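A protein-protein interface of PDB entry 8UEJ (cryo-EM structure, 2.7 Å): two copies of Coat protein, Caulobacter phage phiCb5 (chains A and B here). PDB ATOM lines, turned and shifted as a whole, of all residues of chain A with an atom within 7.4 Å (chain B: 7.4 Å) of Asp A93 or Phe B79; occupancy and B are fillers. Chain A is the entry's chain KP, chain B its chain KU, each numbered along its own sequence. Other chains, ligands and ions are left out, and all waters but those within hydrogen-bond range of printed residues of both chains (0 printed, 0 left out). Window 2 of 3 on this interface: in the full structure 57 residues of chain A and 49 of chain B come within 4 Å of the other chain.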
ATOM      1  N   VAL A  57     -19.611  -6.785  24.398  1.00  0.00           N
ATOM      2  CA  VAL A  57     -20.862  -7.489  24.654  1.00  0.00           C
ATOM      3  C   VAL A  57     -21.358  -8.212  23.401  1.00  0.00           C
ATOM      4  O   VAL A  57     -21.066  -7.819  22.265  1.00  0.00           O
ATOM      5  CB  VAL A  57     -21.921  -6.500  25.168  1.00  0.00           C
ATOM      6  CG1 VAL A  57     -23.227  -7.225  25.459  1.00  0.00           C
ATOM      7  CG2 VAL A  57     -21.405  -5.773  26.406  1.00  0.00           C
ATOM      8  N   TYR A  59     -24.692  -9.428  21.264  1.00  0.00           N
ATOM      9  CA  TYR A  59     -26.070  -9.008  21.037  1.00  0.00           C
ATOM     10  C   TYR A  59     -26.745  -9.913  20.014  1.00  0.00           C
ATOM     11  O   TYR A  59     -26.078 -10.559  19.201  1.00  0.00           O
ATOM     12  CB  TYR A  59     -26.128  -7.559  20.544  1.00  0.00           C
ATOM     13  CG  TYR A  59     -25.902  -6.529  21.620  1.00  0.00           C
ATOM     14  CD1 TYR A  59     -26.928  -6.152  22.473  1.00  0.00           C
ATOM     15  CD2 TYR A  59     -24.663  -5.930  21.783  1.00  0.00           C
ATOM     16  CE1 TYR A  59     -26.723  -5.207  23.454  1.00  0.00           C
ATOM     17  CE2 TYR A  59     -24.451  -4.988  22.760  1.00  0.00           C
ATOM     18  CZ  TYR A  59     -25.481  -4.629  23.592  1.00  0.00           C
ATOM     19  OH  TYR A  59     -25.264  -3.684  24.570  1.00  0.00           O
ATOM     20  N   GLU A  60     -28.078  -9.962  20.066  1.00  0.00           N
ATOM     21  CA  GLU A  60     -28.876 -10.706  19.100  1.00  0.00           C
ATOM     22  C   GLU A  60     -30.072  -9.871  18.659  1.00  0.00           C
ATOM     23  O   GLU A  60     -30.589  -9.048  19.417  1.00  0.00           O
ATOM     24  CB  GLU A  60     -29.346 -12.042  19.685  1.00  0.00           C
ATOM     25  CG  GLU A  60     -30.168 -11.918  20.946  1.00  0.00           C
ATOM     26  CD  GLU A  60     -30.750 -13.247  21.381  1.00  0.00           C
ATOM     27  OE1 GLU A  60     -31.249 -13.334  22.521  1.00  0.00           O
ATOM     28  OE2 GLU A  60     -30.704 -14.207  20.584  1.00  0.00           O
ATOM     29  N   HIS A  89     -31.092  -6.991  21.750  1.00  0.00           N
ATOM     30  CA  HIS A  89     -30.903  -6.960  23.192  1.00  0.00           C
ATOM     31  C   HIS A  89     -29.778  -7.912  23.558  1.00  0.00           C
ATOM     32  O   HIS A  89     -29.413  -8.802  22.786  1.00  0.00           O
ATOM     33  CB  HIS A  89     -32.189  -7.326  23.944  1.00  0.00           C
ATOM     34  CG  HIS A  89     -32.474  -8.795  23.980  1.00  0.00           C
ATOM     35  ND1 HIS A  89     -32.048  -9.610  25.006  1.00  0.00           N
ATOM     36  CD2 HIS A  89     -33.155  -9.594  23.126  1.00  0.00           C
ATOM     37  CE1 HIS A  89     -32.446 -10.848  24.779  1.00  0.00           C
ATOM     38  NE2 HIS A  89     -33.121 -10.866  23.644  1.00  0.00           N
ATOM     39  N   LYS A  90     -29.234  -7.708  24.752  1.00  0.00           N
ATOM     40  CA  LYS A  90     -28.061  -8.449  25.184  1.00  0.00           C
ATOM     41  C   LYS A  90     -28.397  -9.916  25.424  1.00  0.00           C
ATOM     42  O   LYS A  90     -29.488 -10.262  25.886  1.00  0.00           O
ATOM     43  CB  LYS A  90     -27.487  -7.821  26.454  1.00  0.00           C
ATOM     44  CG  LYS A  90     -26.255  -8.520  26.995  1.00  0.00           C
ATOM     45  CD  LYS A  90     -25.775  -7.912  28.304  1.00  0.00           C
ATOM     46  CE  LYS A  90     -26.629  -8.335  29.482  1.00  0.00           C
ATOM     47  NZ  LYS A  90     -25.908  -8.113  30.765  1.00  0.00           N
ATOM     48  N   VAL A  91     -27.436 -10.785  25.111  1.00  0.00           N
ATOM     49  CA  VAL A  91     -27.629 -12.218  25.286  1.00  0.00           C
ATOM     50  C   VAL A  91     -27.693 -12.546  26.771  1.00  0.00           C
ATOM     51  O   VAL A  91     -26.867 -12.082  27.567  1.00  0.00           O
ATOM     52  CB  VAL A  91     -26.501 -12.989  24.582  1.00  0.00           C
ATOM     53  CG1 VAL A  91     -26.469 -14.451  25.029  1.00  0.00           C
ATOM     54  CG2 VAL A  91     -26.660 -12.887  23.068  1.00  0.00           C
ATOM     55  N   GLY A  92     -28.677 -13.357  27.151  1.00  0.00           N
ATOM     56  CA  GLY A  92     -28.876 -13.712  28.540  1.00  0.00           C
ATOM     57  C   GLY A  92     -29.607 -12.686  29.377  1.00  0.00           C
ATOM     58  O   GLY A  92     -29.695 -12.857  30.597  1.00  0.00           O
ATOM     59  N   ASP A  93     -30.132 -11.626  28.769  1.00  0.00           N
ATOM     60  CA  ASP A  93     -30.867 -10.617  29.515  1.00  0.00           C
ATOM     61  C   ASP A  93     -32.243 -11.159  29.907  1.00  0.00           C
ATOM     62  O   ASP A  93     -32.720 -12.168  29.379  1.00  0.00           O
ATOM     63  CB  ASP A  93     -30.987  -9.336  28.681  1.00  0.00           C
ATOM     64  CG  ASP A  93     -31.765  -8.232  29.384  1.00  0.00           C
ATOM     65  OD1 ASP A  93     -32.796  -8.519  30.027  1.00  0.00           O
ATOM     66  OD2 ASP A  93     -31.338  -7.062  29.296  1.00  0.00           O
ATOM     67  N   VAL A  94     -32.890 -10.467  30.841  1.00  0.00           N
ATOM     68  CA  VAL A  94     -34.185 -10.899  31.356  1.00  0.00           C
ATOM     69  C   VAL A  94     -35.242 -10.651  30.289  1.00  0.00           C
ATOM     70  O   VAL A  94     -35.347  -9.544  29.747  1.00  0.00           O
ATOM     71  CB  VAL A  94     -34.521 -10.162  32.662  1.00  0.00           C
ATOM     72  CG1 VAL A  94     -35.941 -10.480  33.112  1.00  0.00           C
ATOM     73  CG2 VAL A  94     -33.515 -10.527  33.748  1.00  0.00           C
ATOM     74  N   SER A  95     -36.024 -11.688  29.979  1.00  0.00           N
ATOM     75  CA  SER A  95     -36.932 -11.622  28.837  1.00  0.00           C
ATOM     76  C   SER A  95     -38.037 -10.591  29.047  1.00  0.00           C
ATOM     77  O   SER A  95     -38.366  -9.831  28.129  1.00  0.00           O
ATOM     78  CB  SER A  95     -37.526 -13.003  28.572  1.00  0.00           C
ATOM     79  OG  SER A  95     -38.244 -13.471  29.700  1.00  0.00           O
ATOM     80  N   ALA A  96     -38.623 -10.549  30.246  1.00  0.00           N
ATOM     81  CA  ALA A  96     -39.746  -9.644  30.481  1.00  0.00           C
ATOM     82  C   ALA A  96     -39.331  -8.186  30.311  1.00  0.00           C
ATOM     83  O   ALA A  96     -40.091  -7.373  29.766  1.00  0.00           O
ATOM     84  CB  ALA A  96     -40.321  -9.876  31.877  1.00  0.00           C
ATOM     85  N   THR A  97     -38.138  -7.831  30.789  1.00  0.00           N
ATOM     86  CA  THR A  97     -37.663  -6.460  30.638  1.00  0.00           C
ATOM     87  C   THR A  97     -37.514  -6.091  29.169  1.00  0.00           C
ATOM     88  O   THR A  97     -37.940  -5.009  28.745  1.00  0.00           O
ATOM     89  CB  THR A  97     -36.333  -6.287  31.371  1.00  0.00           C
ATOM     90  OG1 THR A  97     -36.509  -6.588  32.760  1.00  0.00           O
ATOM     91  CG2 THR A  97     -35.818  -4.861  31.228  1.00  0.00           C
ATOM     92  N   VAL A  98     -36.926  -6.981  28.369  1.00  0.00           N
ATOM     93  CA  VAL A  98     -36.758  -6.695  26.948  1.00  0.00           C
ATOM     94  C   VAL A  98     -38.114  -6.621  26.262  1.00  0.00           C
ATOM     95  O   VAL A  98     -38.278  -5.925  25.254  1.00  0.00           O
ATOM     96  CB  VAL A  98     -35.844  -7.742  26.284  1.00  0.00           C
ATOM     97  CG1 VAL A  98     -35.571  -7.346  24.840  1.00  0.00           C
ATOM     98  CG2 VAL A  98     -34.528  -7.879  27.049  1.00  0.00           C
ATOM     99  N   SER A  99     -39.100  -7.348  26.783  1.00  0.00           N
ATOM    100  CA  SER A  99     -40.430  -7.323  26.188  1.00  0.00           C
ATOM    101  C   SER A  99     -41.173  -6.025  26.482  1.00  0.00           C
ATOM    102  O   SER A  99     -41.868  -5.501  25.599  1.00  0.00           O
ATOM    103  CB  SER A  99     -41.245  -8.512  26.690  1.00  0.00           C
ATOM    104  OG  SER A  99     -42.546  -8.501  26.136  1.00  0.00           O
ATOM    105  N   GLU B  68     -32.562   2.330  25.537  1.00  0.00           N
ATOM    106  CA  GLU B  68     -32.387   2.346  26.984  1.00  0.00           C
ATOM    107  C   GLU B  68     -30.989   1.831  27.289  1.00  0.00           C
ATOM    108  O   GLU B  68     -30.653   0.698  26.925  1.00  0.00           O
ATOM    109  CB  GLU B  68     -33.455   1.488  27.663  1.00  0.00           C
ATOM    110  CG  GLU B  68     -33.659   1.778  29.132  1.00  0.00           C
ATOM    111  CD  GLU B  68     -32.499   1.320  29.987  1.00  0.00           C
ATOM    112  OE1 GLU B  68     -31.866   0.301  29.639  1.00  0.00           O
ATOM    113  OE2 GLU B  68     -32.221   1.977  31.011  1.00  0.00           O
ATOM    114  N   THR B  69     -30.176   2.654  27.946  1.00  0.00           N
ATOM    115  CA  THR B  69     -28.791   2.322  28.249  1.00  0.00           C
ATOM    116  C   THR B  69     -28.601   2.270  29.756  1.00  0.00           C
ATOM    117  O   THR B  69     -29.024   3.183  30.471  1.00  0.00           O
ATOM    118  CB  THR B  69     -27.829   3.337  27.623  1.00  0.00           C
ATOM    119  OG1 THR B  69     -26.479   2.889  27.795  1.00  0.00           O
ATOM    120  CG2 THR B  69     -27.995   4.711  28.259  1.00  0.00           C
ATOM    121  N   VAL B  70     -27.961   1.207  30.232  1.00  0.00           N
ATOM    122  CA  VAL B  70     -27.726   0.988  31.654  1.00  0.00           C
ATOM    123  C   VAL B  70     -26.241   1.183  31.911  1.00  0.00           C
ATOM    124  O   VAL B  70     -25.407   0.485  31.319  1.00  0.00           O
ATOM    125  CB  VAL B  70     -28.184  -0.411  32.093  1.00  0.00           C
ATOM    126  CG1 VAL B  70     -27.919  -0.620  33.571  1.00  0.00           C
ATOM    127  CG2 VAL B  70     -29.659  -0.612  31.777  1.00  0.00           C
ATOM    128  N   TYR B  71     -25.908   2.116  32.801  1.00  0.00           N
ATOM    129  CA  TYR B  71     -24.512   2.427  33.066  1.00  0.00           C
ATOM    130  C   TYR B  71     -23.804   1.246  33.712  1.00  0.00           C
ATOM    131  O   TYR B  71     -24.389   0.484  34.487  1.00  0.00           O
ATOM    132  CB  TYR B  71     -24.391   3.649  33.974  1.00  0.00           C
ATOM    133  CG  TYR B  71     -25.187   4.850  33.523  1.00  0.00           C
ATOM    134  CD1 TYR B  71     -25.924   5.597  34.429  1.00  0.00           C
ATOM    135  CD2 TYR B  71     -25.184   5.255  32.196  1.00  0.00           C
ATOM    136  CE1 TYR B  71     -26.644   6.702  34.019  1.00  0.00           C
ATOM    137  CE2 TYR B  71     -25.901   6.357  31.784  1.00  0.00           C
ATOM    138  CZ  TYR B  71     -26.627   7.075  32.697  1.00  0.00           C
ATOM    139  OH  TYR B  71     -27.344   8.178  32.283  1.00  0.00           O
ATOM    140  N   ALA B  72     -22.520   1.107  33.391  1.00  0.00           N
ATOM    141  CA  ALA B  72     -21.728   0.015  33.930  1.00  0.00           C
ATOM    142  C   ALA B  72     -21.667   0.112  35.447  1.00  0.00           C
ATOM    143  O   ALA B  72     -21.405   1.181  36.005  1.00  0.00           O
ATOM    144  CB  ALA B  72     -20.321   0.044  33.335  1.00  0.00           C
ATOM    145  N   SER B  73     -21.914  -1.012  36.112  1.00  0.00           N
ATOM    146  CA  SER B  73     -21.903  -1.088  37.564  1.00  0.00           C
ATOM    147  C   SER B  73     -21.103  -2.310  37.986  1.00  0.00           C
ATOM    148  O   SER B  73     -21.333  -3.413  37.478  1.00  0.00           O
ATOM    149  CB  SER B  73     -23.324  -1.167  38.123  1.00  0.00           C
ATOM    150  OG  SER B  73     -23.306  -1.471  39.504  1.00  0.00           O
ATOM    151  N   THR B  76     -19.953  -5.502  35.758  1.00  0.00           N
ATOM    152  CA  THR B  76     -20.821  -5.570  34.587  1.00  0.00           C
ATOM    153  C   THR B  76     -20.560  -4.390  33.659  1.00  0.00           C
ATOM    154  O   THR B  76     -20.682  -3.239  34.094  1.00  0.00           O
ATOM    155  CB  THR B  76     -22.282  -5.574  35.019  1.00  0.00           C
ATOM    156  OG1 THR B  76     -22.531  -6.688  35.884  1.00  0.00           O
ATOM    157  CG2 THR B  76     -23.200  -5.662  33.806  1.00  0.00           C
ATOM    158  N   PRO B  77     -20.209  -4.611  32.395  1.00  0.00           N
ATOM    159  CA  PRO B  77     -20.019  -3.485  31.477  1.00  0.00           C
ATOM    160  C   PRO B  77     -21.349  -2.893  31.033  1.00  0.00           C
ATOM    161  O   PRO B  77     -22.423  -3.461  31.234  1.00  0.00           O
ATOM    162  CB  PRO B  77     -19.255  -4.107  30.308  1.00  0.00           C
ATOM    163  CG  PRO B  77     -19.664  -5.525  30.314  1.00  0.00           C
ATOM    164  CD  PRO B  77     -19.879  -5.896  31.754  1.00  0.00           C
ATOM    165  N   GLU B  78     -21.255  -1.719  30.415  1.00  0.00           N
ATOM    166  CA  GLU B  78     -22.438  -1.009  29.951  1.00  0.00           C
ATOM    167  C   GLU B  78     -23.100  -1.761  28.802  1.00  0.00           C
ATOM    168  O   GLU B  78     -22.425  -2.352  27.954  1.00  0.00           O
ATOM    169  CB  GLU B  78     -22.049   0.401  29.504  1.00  0.00           C
ATOM    170  CG  GLU B  78     -23.202   1.285  29.069  1.00  0.00           C
ATOM    171  CD  GLU B  78     -22.738   2.676  28.693  1.00  0.00           C
ATOM    172  OE1 GLU B  78     -21.516   2.929  28.760  1.00  0.00           O
ATOM    173  OE2 GLU B  78     -23.590   3.516  28.337  1.00  0.00           O
ATOM    174  N   PHE B  79     -24.431  -1.737  28.776  1.00  0.00           N
ATOM    175  CA  PHE B  79     -25.182  -2.358  27.694  1.00  0.00           C
ATOM    176  C   PHE B  79     -26.456  -1.563  27.451  1.00  0.00           C
ATOM    177  O   PHE B  79     -26.822  -0.678  28.228  1.00  0.00           O
ATOM    178  CB  PHE B  79     -25.505  -3.827  27.992  1.00  0.00           C
ATOM    179  CG  PHE B  79     -26.355  -4.033  29.212  1.00  0.00           C
ATOM    180  CD1 PHE B  79     -25.799  -3.987  30.472  1.00  0.00           C
ATOM    181  CD2 PHE B  79     -27.708  -4.284  29.098  1.00  0.00           C
ATOM    182  CE1 PHE B  79     -26.572  -4.181  31.591  1.00  0.00           C
ATOM    183  CE2 PHE B  79     -28.483  -4.478  30.218  1.00  0.00           C
ATOM    184  CZ  PHE B  79     -27.914  -4.426  31.465  1.00  0.00           C
ATOM    185  N   VAL B  80     -27.131  -1.895  26.349  1.00  0.00           N
ATOM    186  CA  VAL B  80     -28.246  -1.111  25.839  1.00  0.00           C
ATOM    187  C   VAL B  80     -29.408  -2.037  25.499  1.00  0.00           C
ATOM    188  O   VAL B  80     -29.251  -3.251  25.357  1.00  0.00           O
ATOM    189  CB  VAL B  80     -27.840  -0.294  24.594  1.00  0.00           C
ATOM    190  CG1 VAL B  80     -26.555   0.495  24.863  1.00  0.00           C
ATOM    191  CG2 VAL B  80     -27.670  -1.211  23.389  1.00  0.00           C
ATOM    192  N   ARG B  81     -30.590  -1.437  25.378  1.00  0.00           N
ATOM    193  CA  ARG B  81     -31.792  -2.121  24.909  1.00  0.00           C
ATOM    194  C   ARG B  81     -32.592  -1.142  24.063  1.00  0.00           C
ATOM    195  O   ARG B  81     -32.977  -0.078  24.556  1.00  0.00           O
ATOM    196  CB  ARG B  81     -32.646  -2.634  26.076  1.00  0.00           C
ATOM    197  CG  ARG B  81     -32.039  -3.778  26.887  1.00  0.00           C
ATOM    198  CD  ARG B  81     -33.051  -4.350  27.891  1.00  0.00           C
ATOM    199  NE  ARG B  81     -33.454  -3.401  28.923  1.00  0.00           N
ATOM    200  CZ  ARG B  81     -32.817  -3.235  30.076  1.00  0.00           C
ATOM    201  NH1 ARG B  81     -31.752  -3.960  30.393  1.00  0.00           N
ATOM    202  NH2 ARG B  81     -33.266  -2.329  30.943  1.00  0.00           N
ATOM    203  N   ILE B 118     -38.586 -13.949  21.488  1.00  0.00           N
ATOM    204  CA  ILE B 118     -37.450 -14.210  22.366  1.00  0.00           C
ATOM    205  C   ILE B 118     -37.191 -15.704  22.454  1.00  0.00           C
ATOM    206  O   ILE B 118     -36.055 -16.134  22.681  1.00  0.00           O
ATOM    207  CB  ILE B 118     -37.684 -13.592  23.758  1.00  0.00           C
ATOM    208  CG1 ILE B 118     -37.885 -12.075  23.651  1.00  0.00           C
ATOM    209  CG2 ILE B 118     -36.526 -13.925  24.686  1.00  0.00           C
ATOM    210  CD1 ILE B 118     -36.735 -11.328  22.993  1.00  0.00           C
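OH of Tyr A59 sits at hydrogen-bond distance from N of Val B80. The side-chain carboxylate (OD2) of Asp A93 is in salt-bridge range of the guanidinium group (NH1) of Arg B81, 3.3 Å away.
N of His A89 sits at hydrogen-bond distance from O of Glu A60 (3.2 Å). The side-chain carboxylate (OE1) of Glu B68 is in salt-bridge range of the guanidinium group (NH2) of Arg B81, at 3.3 Å. The side-chain carboxylate (OE2) of Glu B78 sits at hydrogen-bond distance from the side-chain hydroxyl (OG1) of Thr B69. The backbone NH of Val B70 is in hydrogen-bond range of the backbone carbonyl oxygen of Phe B79 (3.0 Å).
Glu B78 touches Val A57. OH of Tyr A59 touches CA of Phe B79, at 3.4 Å. His A89 touches Ile B118 (NE2 to CD1, 3.7 Å). OD2 of Asp A93 touches CE2 of Phe B79, at 3.96 Å. Thr A97 touches Arg B81. CG2 of Val A98 touches CD of Arg B81, at 3.9 Å.
Phe B79 touches two residues of chain A. Of the printed residues of chain A, Val B80 touches Tyr A59. Of the printed residues of chain A, Glu B78 touches Val A57. Of the printed residues of chain B, Val A57 touches Glu B78. Of the printed residues of chain B, Tyr A59 touches Phe B79 (3.4 Å) and Val B80 (3.1 Å). Val A91 touches none of the printed residues of chain B. The nearest residue of chain B that does not touch Asp A93 is Val B80 (5.9 Å). The nearest residue of chain A that does not touch Phe B79 is Lys A90 (4.03 Å).
Along chain A the printed residues that touch a printed residue of chain B span positions 57 to 98. Hydrophobic or aromatic side chains of chain B that line the printed part of chain A: Phe B79, Val B80 and Ile B118. Among the printed residues, Asp or Glu carboxylates within 4 Å of a Lys or Arg side-chain nitrogen of the other chain: Asp A93 with Arg B81 (3.3 Å).
No position is printed for both chains. Of the 8 pairs that touch across the chains among the printed residues, none has its exchanged pair printed and touching as well.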
